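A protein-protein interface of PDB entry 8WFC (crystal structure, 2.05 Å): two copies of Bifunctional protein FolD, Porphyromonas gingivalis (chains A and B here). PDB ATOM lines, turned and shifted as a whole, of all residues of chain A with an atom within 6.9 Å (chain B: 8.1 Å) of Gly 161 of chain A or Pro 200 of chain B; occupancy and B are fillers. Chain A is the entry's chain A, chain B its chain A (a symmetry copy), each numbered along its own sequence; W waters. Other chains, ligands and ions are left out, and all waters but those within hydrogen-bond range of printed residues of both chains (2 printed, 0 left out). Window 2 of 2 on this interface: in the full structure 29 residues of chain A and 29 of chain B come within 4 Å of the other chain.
Printed residues of chain B that touch a printed residue of chain A: His 196, Arg 198, Thr 199 and Pro 200.
Hydrophobic or aromatic side chains of chain B that line the printed part of chain A: His 196 and Pro 200.
Among the printed residues, 6 pairs touch across the chains.
Among the printed residues, no Asp or Glu carboxylate lies within 4 Å of a Lys or Arg side-chain nitrogen of the other chain.
NE2 of His 196 of chain B is in hydrogen-bond range of O of Cys 190 of chain A (2.7 Å).
The side-chain hydroxyl (OG1) of Thr 191 of chain A lies within hydrogen-bond range of the side-chain hydroxyl (OG1) of Thr 199 of chain B, 2.7 Å away.
No position is printed for both chains.
Of the 6 pairs that touch across the chains among the printed residues, none has its exchanged pair printed and touching as well.
Among the printed residues, merely in contact across the chains: Gly 161 of chain A with Arg 198 of chain B (3.2 Å), Gly 161 of chain A with Pro 200 of chain B (3.6 Å), Asp 189 of chain A with His 196 of chain B (3.5 Å) and Asp 189 of chain A with Arg 198 of chain B (3.7 Å).
Of chain B, only Arg 198 and Pro 200 come within 4 Å of Gly 161 of chain A.
Of the printed residues of chain B, Cys 190 of chain A touches His 196.
Printed residues of chain A within 4 Å of Arg 198 of chain B: Gly 161 (3.2 Å) and Asp 189 (3.7 Å).
Of chain A, only Gly 161 comes within 4 Å of Pro 200 of chain B.
The nearest residue of chain A that does not touch Pro 200 of chain B is Thr 191 of chain A (4.3 Å).
The nearest printed residue of chain B that does not touch Asp 189 of chain A is Thr 199 of chain B (5.7 Å).
Water W2 bridges OD2 of Asp 189 of chain A and NE of Arg 198 of chain B.
Water W1 lies within hydrogen-bond range of ND2 of Asn 201 of chain B and ND1 of His 163 of chain A.
The backbone NH of His 196 of chain B is in hydrogen-bond range of the side-chain hydroxyl of Thr 199 of chain B (2.9 Å).
A ring nitrogen (ND1) of His 196 of chain B lies within hydrogen-bond range of the backbone NH (N) of Arg 198 of chain B.
N of Gly 161 of chain A lies within hydrogen-bond range of O of Asp 189 of chain A, 2.9 Å away.
The side-chain sulfur of Cys 190 of chain A is in hydrogen-bond range of the backbone carbonyl oxygen of Thr 159 of chain A, at 3.5 Å.
O of Lys 162 of chain A sits at hydrogen-bond distance from N of Thr 191 of chain A (2.8 Å).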
ATOM      1  N   PRO A 158      29.442 -29.402  -9.509  1.00  0.00           N
ATOM      2  CA  PRO A 158      29.393 -27.943  -9.351  1.00  0.00           C
ATOM      3  C   PRO A 158      28.558 -27.316 -10.464  1.00  0.00           C
ATOM      4  O   PRO A 158      28.751 -27.620 -11.648  1.00  0.00           O
ATOM      5  CB  PRO A 158      30.868 -27.533  -9.437  1.00  0.00           C
ATOM      6  CG  PRO A 158      31.638 -28.790  -9.081  1.00  0.00           C
ATOM      7  CD  PRO A 158      30.822 -29.901  -9.653  1.00  0.00           C
ATOM      8  N   THR A 159      27.606 -26.453 -10.076  1.00  0.00           N
ATOM      9  CA  THR A 159      26.742 -25.788 -11.051  1.00  0.00           C
ATOM     10  C   THR A 159      26.690 -24.281 -10.836  1.00  0.00           C
ATOM     11  O   THR A 159      26.413 -23.529 -11.779  1.00  0.00           O
ATOM     12  CB  THR A 159      25.307 -26.333 -11.020  1.00  0.00           C
ATOM     13  OG1 THR A 159      24.758 -26.167  -9.707  1.00  0.00           O
ATOM     14  CG2 THR A 159      25.240 -27.794 -11.424  1.00  0.00           C
ATOM     15  N   ARG A 160      26.916 -23.824  -9.607  1.00  0.00           N
ATOM     16  CA  ARG A 160      26.838 -22.394  -9.346  1.00  0.00           C
ATOM     17  C   ARG A 160      27.858 -21.643 -10.188  1.00  0.00           C
ATOM     18  O   ARG A 160      29.037 -22.019 -10.241  1.00  0.00           O
ATOM     19  CB  ARG A 160      27.070 -22.101  -7.869  1.00  0.00           C
ATOM     20  CG  ARG A 160      27.087 -20.627  -7.564  1.00  0.00           C
ATOM     21  CD  ARG A 160      27.662 -20.362  -6.178  1.00  0.00           C
ATOM     22  NE  ARG A 160      26.680 -20.643  -5.141  1.00  0.00           N
ATOM     23  CZ  ARG A 160      26.921 -21.333  -4.037  1.00  0.00           C
ATOM     24  NH1 ARG A 160      28.140 -21.825  -3.795  1.00  0.00           N
ATOM     25  NH2 ARG A 160      25.934 -21.504  -3.159  1.00  0.00           N
ATOM     26  N   GLY A 161      27.397 -20.586 -10.853  1.00  0.00           N
ATOM     27  CA  GLY A 161      28.273 -19.772 -11.672  1.00  0.00           C
ATOM     28  C   GLY A 161      28.716 -20.406 -12.967  1.00  0.00           C
ATOM     29  O   GLY A 161      29.557 -19.832 -13.665  1.00  0.00           O
ATOM     30  N   LYS A 162      28.181 -21.567 -13.311  1.00  0.00           N
ATOM     31  CA  LYS A 162      28.571 -22.297 -14.506  1.00  0.00           C
ATOM     32  C   LYS A 162      27.630 -21.952 -15.655  1.00  0.00           C
ATOM     33  O   LYS A 162      26.451 -21.650 -15.441  1.00  0.00           O
ATOM     34  CB  LYS A 162      28.543 -23.804 -14.243  1.00  0.00           C
ATOM     35  CG  LYS A 162      29.448 -24.242 -13.100  1.00  0.00           C
ATOM     36  CD  LYS A 162      30.920 -24.118 -13.489  1.00  0.00           C
ATOM     37  CE  LYS A 162      31.831 -24.601 -12.357  1.00  0.00           C
ATOM     38  NZ  LYS A 162      33.260 -24.319 -12.646  1.00  0.00           N
ATOM     39  N   HIS A 163      28.159 -22.008 -16.878  1.00  0.00           N
ATOM     40  CA  HIS A 163      27.379 -21.713 -18.076  1.00  0.00           C
ATOM     41  C   HIS A 163      26.730 -23.006 -18.566  1.00  0.00           C
ATOM     42  O   HIS A 163      27.422 -23.923 -19.016  1.00  0.00           O
ATOM     43  CB  HIS A 163      28.255 -21.089 -19.163  1.00  0.00           C
ATOM     44  CG  HIS A 163      27.483 -20.617 -20.359  1.00  0.00           C
ATOM     45  ND1 HIS A 163      28.040 -20.513 -21.617  1.00  0.00           N
ATOM     46  CD2 HIS A 163      26.193 -20.221 -20.486  1.00  0.00           C
ATOM     47  CE1 HIS A 163      27.124 -20.077 -22.468  1.00  0.00           C
ATOM     48  NE2 HIS A 163      25.995 -19.890 -21.808  1.00  0.00           N
ATOM     49  N   GLU A 186      22.411 -25.007  -5.295  1.00  0.00           N
ATOM     50  CA  GLU A 186      22.899 -26.064  -6.164  1.00  0.00           C
ATOM     51  C   GLU A 186      22.092 -27.341  -5.957  1.00  0.00           C
ATOM     52  O   GLU A 186      21.696 -27.639  -4.825  1.00  0.00           O
ATOM     53  CB  GLU A 186      24.389 -26.345  -5.908  1.00  0.00           C
ATOM     54  CG  GLU A 186      25.330 -25.354  -6.579  1.00  0.00           C
ATOM     55  CD  GLU A 186      26.814 -25.607  -6.267  1.00  0.00           C
ATOM     56  OE1 GLU A 186      27.178 -25.741  -5.075  1.00  0.00           O
ATOM     57  OE2 GLU A 186      27.612 -25.682  -7.229  1.00  0.00           O
ATOM     58  N   GLY A 188      21.880 -25.700  -9.669  1.00  0.00           N
ATOM     59  CA  GLY A 188      21.248 -24.460 -10.081  1.00  0.00           C
ATOM     60  C   GLY A 188      22.252 -23.321 -10.038  1.00  0.00           C
ATOM     61  O   GLY A 188      23.455 -23.543  -9.992  1.00  0.00           O
ATOM     62  N   ASP A 189      21.731 -22.099 -10.053  1.00  0.00           N
ATOM     63  CA  ASP A 189      22.562 -20.892 -10.167  1.00  0.00           C
ATOM     64  C   ASP A 189      23.455 -20.940 -11.410  1.00  0.00           C
ATOM     65  O   ASP A 189      24.534 -20.332 -11.444  1.00  0.00           O
ATOM     66  CB  ASP A 189      23.403 -20.657  -8.897  1.00  0.00           C
ATOM     67  CG  ASP A 189      22.649 -19.866  -7.825  1.00  0.00           C
ATOM     68  OD1 ASP A 189      21.804 -19.018  -8.184  1.00  0.00           O
ATOM     69  OD2 ASP A 189      22.905 -20.081  -6.615  1.00  0.00           O
ATOM     70  N   CYS A 190      23.006 -21.650 -12.448  1.00  0.00           N
ATOM     71  CA  CYS A 190      23.664 -21.612 -13.749  1.00  0.00           C
ATOM     72  C   CYS A 190      23.294 -20.349 -14.522  1.00  0.00           C
ATOM     73  O   CYS A 190      22.176 -19.832 -14.420  1.00  0.00           O
ATOM     74  CB  CYS A 190      23.269 -22.831 -14.579  1.00  0.00           C
ATOM     75  SG  CYS A 190      23.805 -24.367 -13.904  1.00  0.00           S
ATOM     76  N   THR A 191      24.232 -19.865 -15.338  1.00  0.00           N
ATOM     77  CA  THR A 191      23.853 -18.944 -16.411  1.00  0.00           C
ATOM     78  C   THR A 191      23.345 -19.803 -17.566  1.00  0.00           C
ATOM     79  O   THR A 191      24.033 -20.732 -17.985  1.00  0.00           O
ATOM     80  CB  THR A 191      25.044 -18.090 -16.848  1.00  0.00           C
ATOM     81  OG1 THR A 191      25.550 -17.363 -15.718  1.00  0.00           O
ATOM     82  CG2 THR A 191      24.642 -17.104 -17.967  1.00  0.00           C
ATOM     83  N   ASP A 210      30.017 -24.913 -19.744  1.00  0.00           N
ATOM     84  CA  ASP A 210      30.453 -25.856 -18.722  1.00  0.00           C
ATOM     85  C   ASP A 210      29.546 -27.079 -18.667  1.00  0.00           C
ATOM     86  O   ASP A 210      30.009 -28.183 -18.359  1.00  0.00           O
ATOM     87  CB  ASP A 210      30.476 -25.155 -17.372  1.00  0.00           C
ATOM     88  CG  ASP A 210      31.315 -23.884 -17.413  1.00  0.00           C
ATOM     89  OD1 ASP A 210      32.515 -24.008 -17.684  1.00  0.00           O
ATOM     90  OD2 ASP A 210      30.777 -22.774 -17.233  1.00  0.00           O
ATOM     91  N   CYS B 195      21.093 -14.031 -17.321  1.00  0.00           N
ATOM     92  CA  CYS B 195      22.174 -13.732 -16.398  1.00  0.00           C
ATOM     93  C   CYS B 195      21.602 -13.316 -15.043  1.00  0.00           C
ATOM     94  O   CYS B 195      20.490 -12.797 -14.948  1.00  0.00           O
ATOM     95  CB  CYS B 195      23.040 -12.597 -16.951  1.00  0.00           C
ATOM     96  SG  CYS B 195      23.897 -13.000 -18.456  1.00  0.00           S
ATOM     97  N   HIS B 196      22.393 -13.495 -13.987  1.00  0.00           N
ATOM     98  CA  HIS B 196      21.932 -13.096 -12.653  1.00  0.00           C
ATOM     99  C   HIS B 196      23.158 -12.875 -11.769  1.00  0.00           C
ATOM    100  O   HIS B 196      24.290 -12.808 -12.261  1.00  0.00           O
ATOM    101  CB  HIS B 196      20.979 -14.164 -12.101  1.00  0.00           C
ATOM    102  CG  HIS B 196      21.533 -15.546 -12.244  1.00  0.00           C
ATOM    103  ND1 HIS B 196      22.605 -15.990 -11.500  1.00  0.00           N
ATOM    104  CD2 HIS B 196      21.216 -16.557 -13.093  1.00  0.00           C
ATOM    105  CE1 HIS B 196      22.912 -17.224 -11.865  1.00  0.00           C
ATOM    106  NE2 HIS B 196      22.085 -17.593 -12.832  1.00  0.00           N
ATOM    107  N   SER B 197      22.944 -12.755 -10.462  1.00  0.00           N
ATOM    108  CA  SER B 197      24.031 -12.430  -9.502  1.00  0.00           C
ATOM    109  C   SER B 197      25.197 -13.428  -9.526  1.00  0.00           C
ATOM    110  O   SER B 197      26.269 -13.020  -9.190  1.00  0.00           O
ATOM    111  CB  SER B 197      23.506 -12.202  -8.120  1.00  0.00           C
ATOM    112  OG  SER B 197      23.044 -13.401  -7.573  1.00  0.00           O
ATOM    113  N   ARG B 198      24.970 -14.675  -9.920  1.00  0.00           N
ATOM    114  CA  ARG B 198      26.051 -15.686  -9.954  1.00  0.00           C
ATOM    115  C   ARG B 198      26.687 -15.793 -11.342  1.00  0.00           C
ATOM    116  O   ARG B 198      27.540 -16.617 -11.498  1.00  0.00           O
ATOM    117  CB  ARG B 198      25.539 -17.031  -9.461  1.00  0.00           C
ATOM    118  CG  ARG B 198      24.924 -16.986  -8.075  1.00  0.00           C
ATOM    119  CD  ARG B 198      25.854 -16.426  -7.034  1.00  0.00           C
ATOM    120  NE  ARG B 198      25.116 -16.260  -5.804  1.00  0.00           N
ATOM    121  CZ  ARG B 198      25.525 -15.609  -4.733  1.00  0.00           C
ATOM    122  NH1 ARG B 198      24.730 -15.541  -3.686  1.00  0.00           N
ATOM    123  NH2 ARG B 198      26.714 -15.045  -4.695  1.00  0.00           N
ATOM    124  N   THR B 199      26.238 -15.000 -12.299  1.00  0.00           N
ATOM    125  CA  THR B 199      26.867 -15.005 -13.635  1.00  0.00           C
ATOM    126  C   THR B 199      28.207 -14.296 -13.475  1.00  0.00           C
ATOM    127  O   THR B 199      28.189 -13.142 -13.198  1.00  0.00           O
ATOM    128  CB  THR B 199      26.000 -14.291 -14.668  1.00  0.00           C
ATOM    129  OG1 THR B 199      24.746 -14.954 -14.745  1.00  0.00           O
ATOM    130  CG2 THR B 199      26.661 -14.208 -16.023  1.00  0.00           C
ATOM    131  N   PRO B 200      29.352 -14.959 -13.679  1.00  0.00           N
ATOM    132  CA  PRO B 200      30.644 -14.333 -13.453  1.00  0.00           C
ATOM    133  C   PRO B 200      31.164 -13.402 -14.550  1.00  0.00           C
ATOM    134  O   PRO B 200      32.018 -12.654 -14.247  1.00  0.00           O
ATOM    135  CB  PRO B 200      31.586 -15.532 -13.424  1.00  0.00           C
ATOM    136  CG  PRO B 200      30.950 -16.507 -14.353  1.00  0.00           C
ATOM    137  CD  PRO B 200      29.465 -16.310 -14.165  1.00  0.00           C
ATOM    138  N   ASN B 201      30.578 -13.432 -15.742  1.00  0.00           N
ATOM    139  CA  ASN B 201      31.155 -12.679 -16.858  1.00  0.00           C
ATOM    140  C   ASN B 201      30.080 -11.885 -17.587  1.00  0.00           C
ATOM    141  O   ASN B 201      29.946 -11.951 -18.811  1.00  0.00           O
ATOM    142  CB  ASN B 201      31.870 -13.615 -17.831  1.00  0.00           C
ATOM    143  CG  ASN B 201      30.949 -14.718 -18.368  1.00  0.00           C
ATOM    144  OD1 ASN B 201      29.934 -15.067 -17.737  1.00  0.00           O
ATOM    145  ND2 ASN B 201      31.278 -15.249 -19.554  1.00  0.00           N
ATOM    146  N   ILE B 202      29.307 -11.090 -16.843  1.00  0.00           N
ATOM    147  CA  ILE B 202      28.145 -10.440 -17.450  1.00  0.00           C
ATOM    148  C   ILE B 202      28.564  -9.505 -18.586  1.00  0.00           C
ATOM    149  O   ILE B 202      27.899  -9.442 -19.629  1.00  0.00           O
ATOM    150  CB  ILE B 202      27.328  -9.701 -16.379  1.00  0.00           C
ATOM    151  CG1 ILE B 202      26.641 -10.718 -15.455  1.00  0.00           C
ATOM    152  CG2 ILE B 202      26.290  -8.805 -17.034  1.00  0.00           C
ATOM    153  CD1 ILE B 202      25.886 -10.091 -14.285  1.00  0.00           C
ATOM    154  N   LYS B 203      29.674  -8.785 -18.416  1.00  0.00           N
ATOM    155  CA  LYS B 203      30.172  -7.854 -19.467  1.00  0.00           C
ATOM    156  C   LYS B 203      30.452  -8.630 -20.756  1.00  0.00           C
ATOM    157  O   LYS B 203      29.985  -8.219 -21.791  1.00  0.00           O
ATOM    158  CB  LYS B 203      31.428  -7.100 -19.032  1.00  0.00           C
ATOM    159  CG  LYS B 203      32.086  -6.270 -20.120  1.00  0.00           C
ATOM    160  CD  LYS B 203      33.127  -5.321 -19.592  1.00  0.00           C
ATOM    161  CE  LYS B 203      34.061  -4.752 -20.638  1.00  0.00           C
ATOM    162  NZ  LYS B 203      35.004  -3.784 -20.042  1.00  0.00           N
ATOM    163  N   GLU B 204      31.167  -9.742 -20.644  1.00  0.00           N
ATOM    164  CA  GLU B 204      31.512 -10.603 -21.798  1.00  0.00           C
ATOM    165  C   GLU B 204      30.222 -11.061 -22.489  1.00  0.00           C
ATOM    166  O   GLU B 204      30.153 -11.010 -23.692  1.00  0.00           O
ATOM    167  CB  GLU B 204      32.375 -11.765 -21.316  1.00  0.00           C
ATOM    168  CG  GLU B 204      32.916 -12.620 -22.441  1.00  0.00           C
ATOM    169  CD  GLU B 204      33.722 -13.853 -22.060  1.00  0.00           C
ATOM    170  OE1 GLU B 204      34.411 -14.378 -22.931  1.00  0.00           O
ATOM    171  OE2 GLU B 204      33.651 -14.285 -20.922  1.00  0.00           O
ATOM    172  N   VAL B 205      29.235 -11.463 -21.709  1.00  0.00           N
ATOM    173  CA  VAL B 205      27.944 -11.931 -22.265  1.00  0.00           C
ATOM    174  C   VAL B 205      27.234 -10.790 -22.991  1.00  0.00           C
ATOM    175  O   VAL B 205      26.790 -11.010 -24.095  1.00  0.00           O
ATOM    176  CB  VAL B 205      27.081 -12.583 -21.176  1.00  0.00           C
ATOM    177  CG1 VAL B 205      25.717 -12.966 -21.716  1.00  0.00           C
ATOM    178  CG2 VAL B 205      27.787 -13.787 -20.592  1.00  0.00           C
HETATM  179  O   HOH W   1      30.070 -17.889 -20.818  1.00  0.00           O
HETATM  180  O   HOH W   2      22.359 -17.414  -5.463  1.00  0.00           O
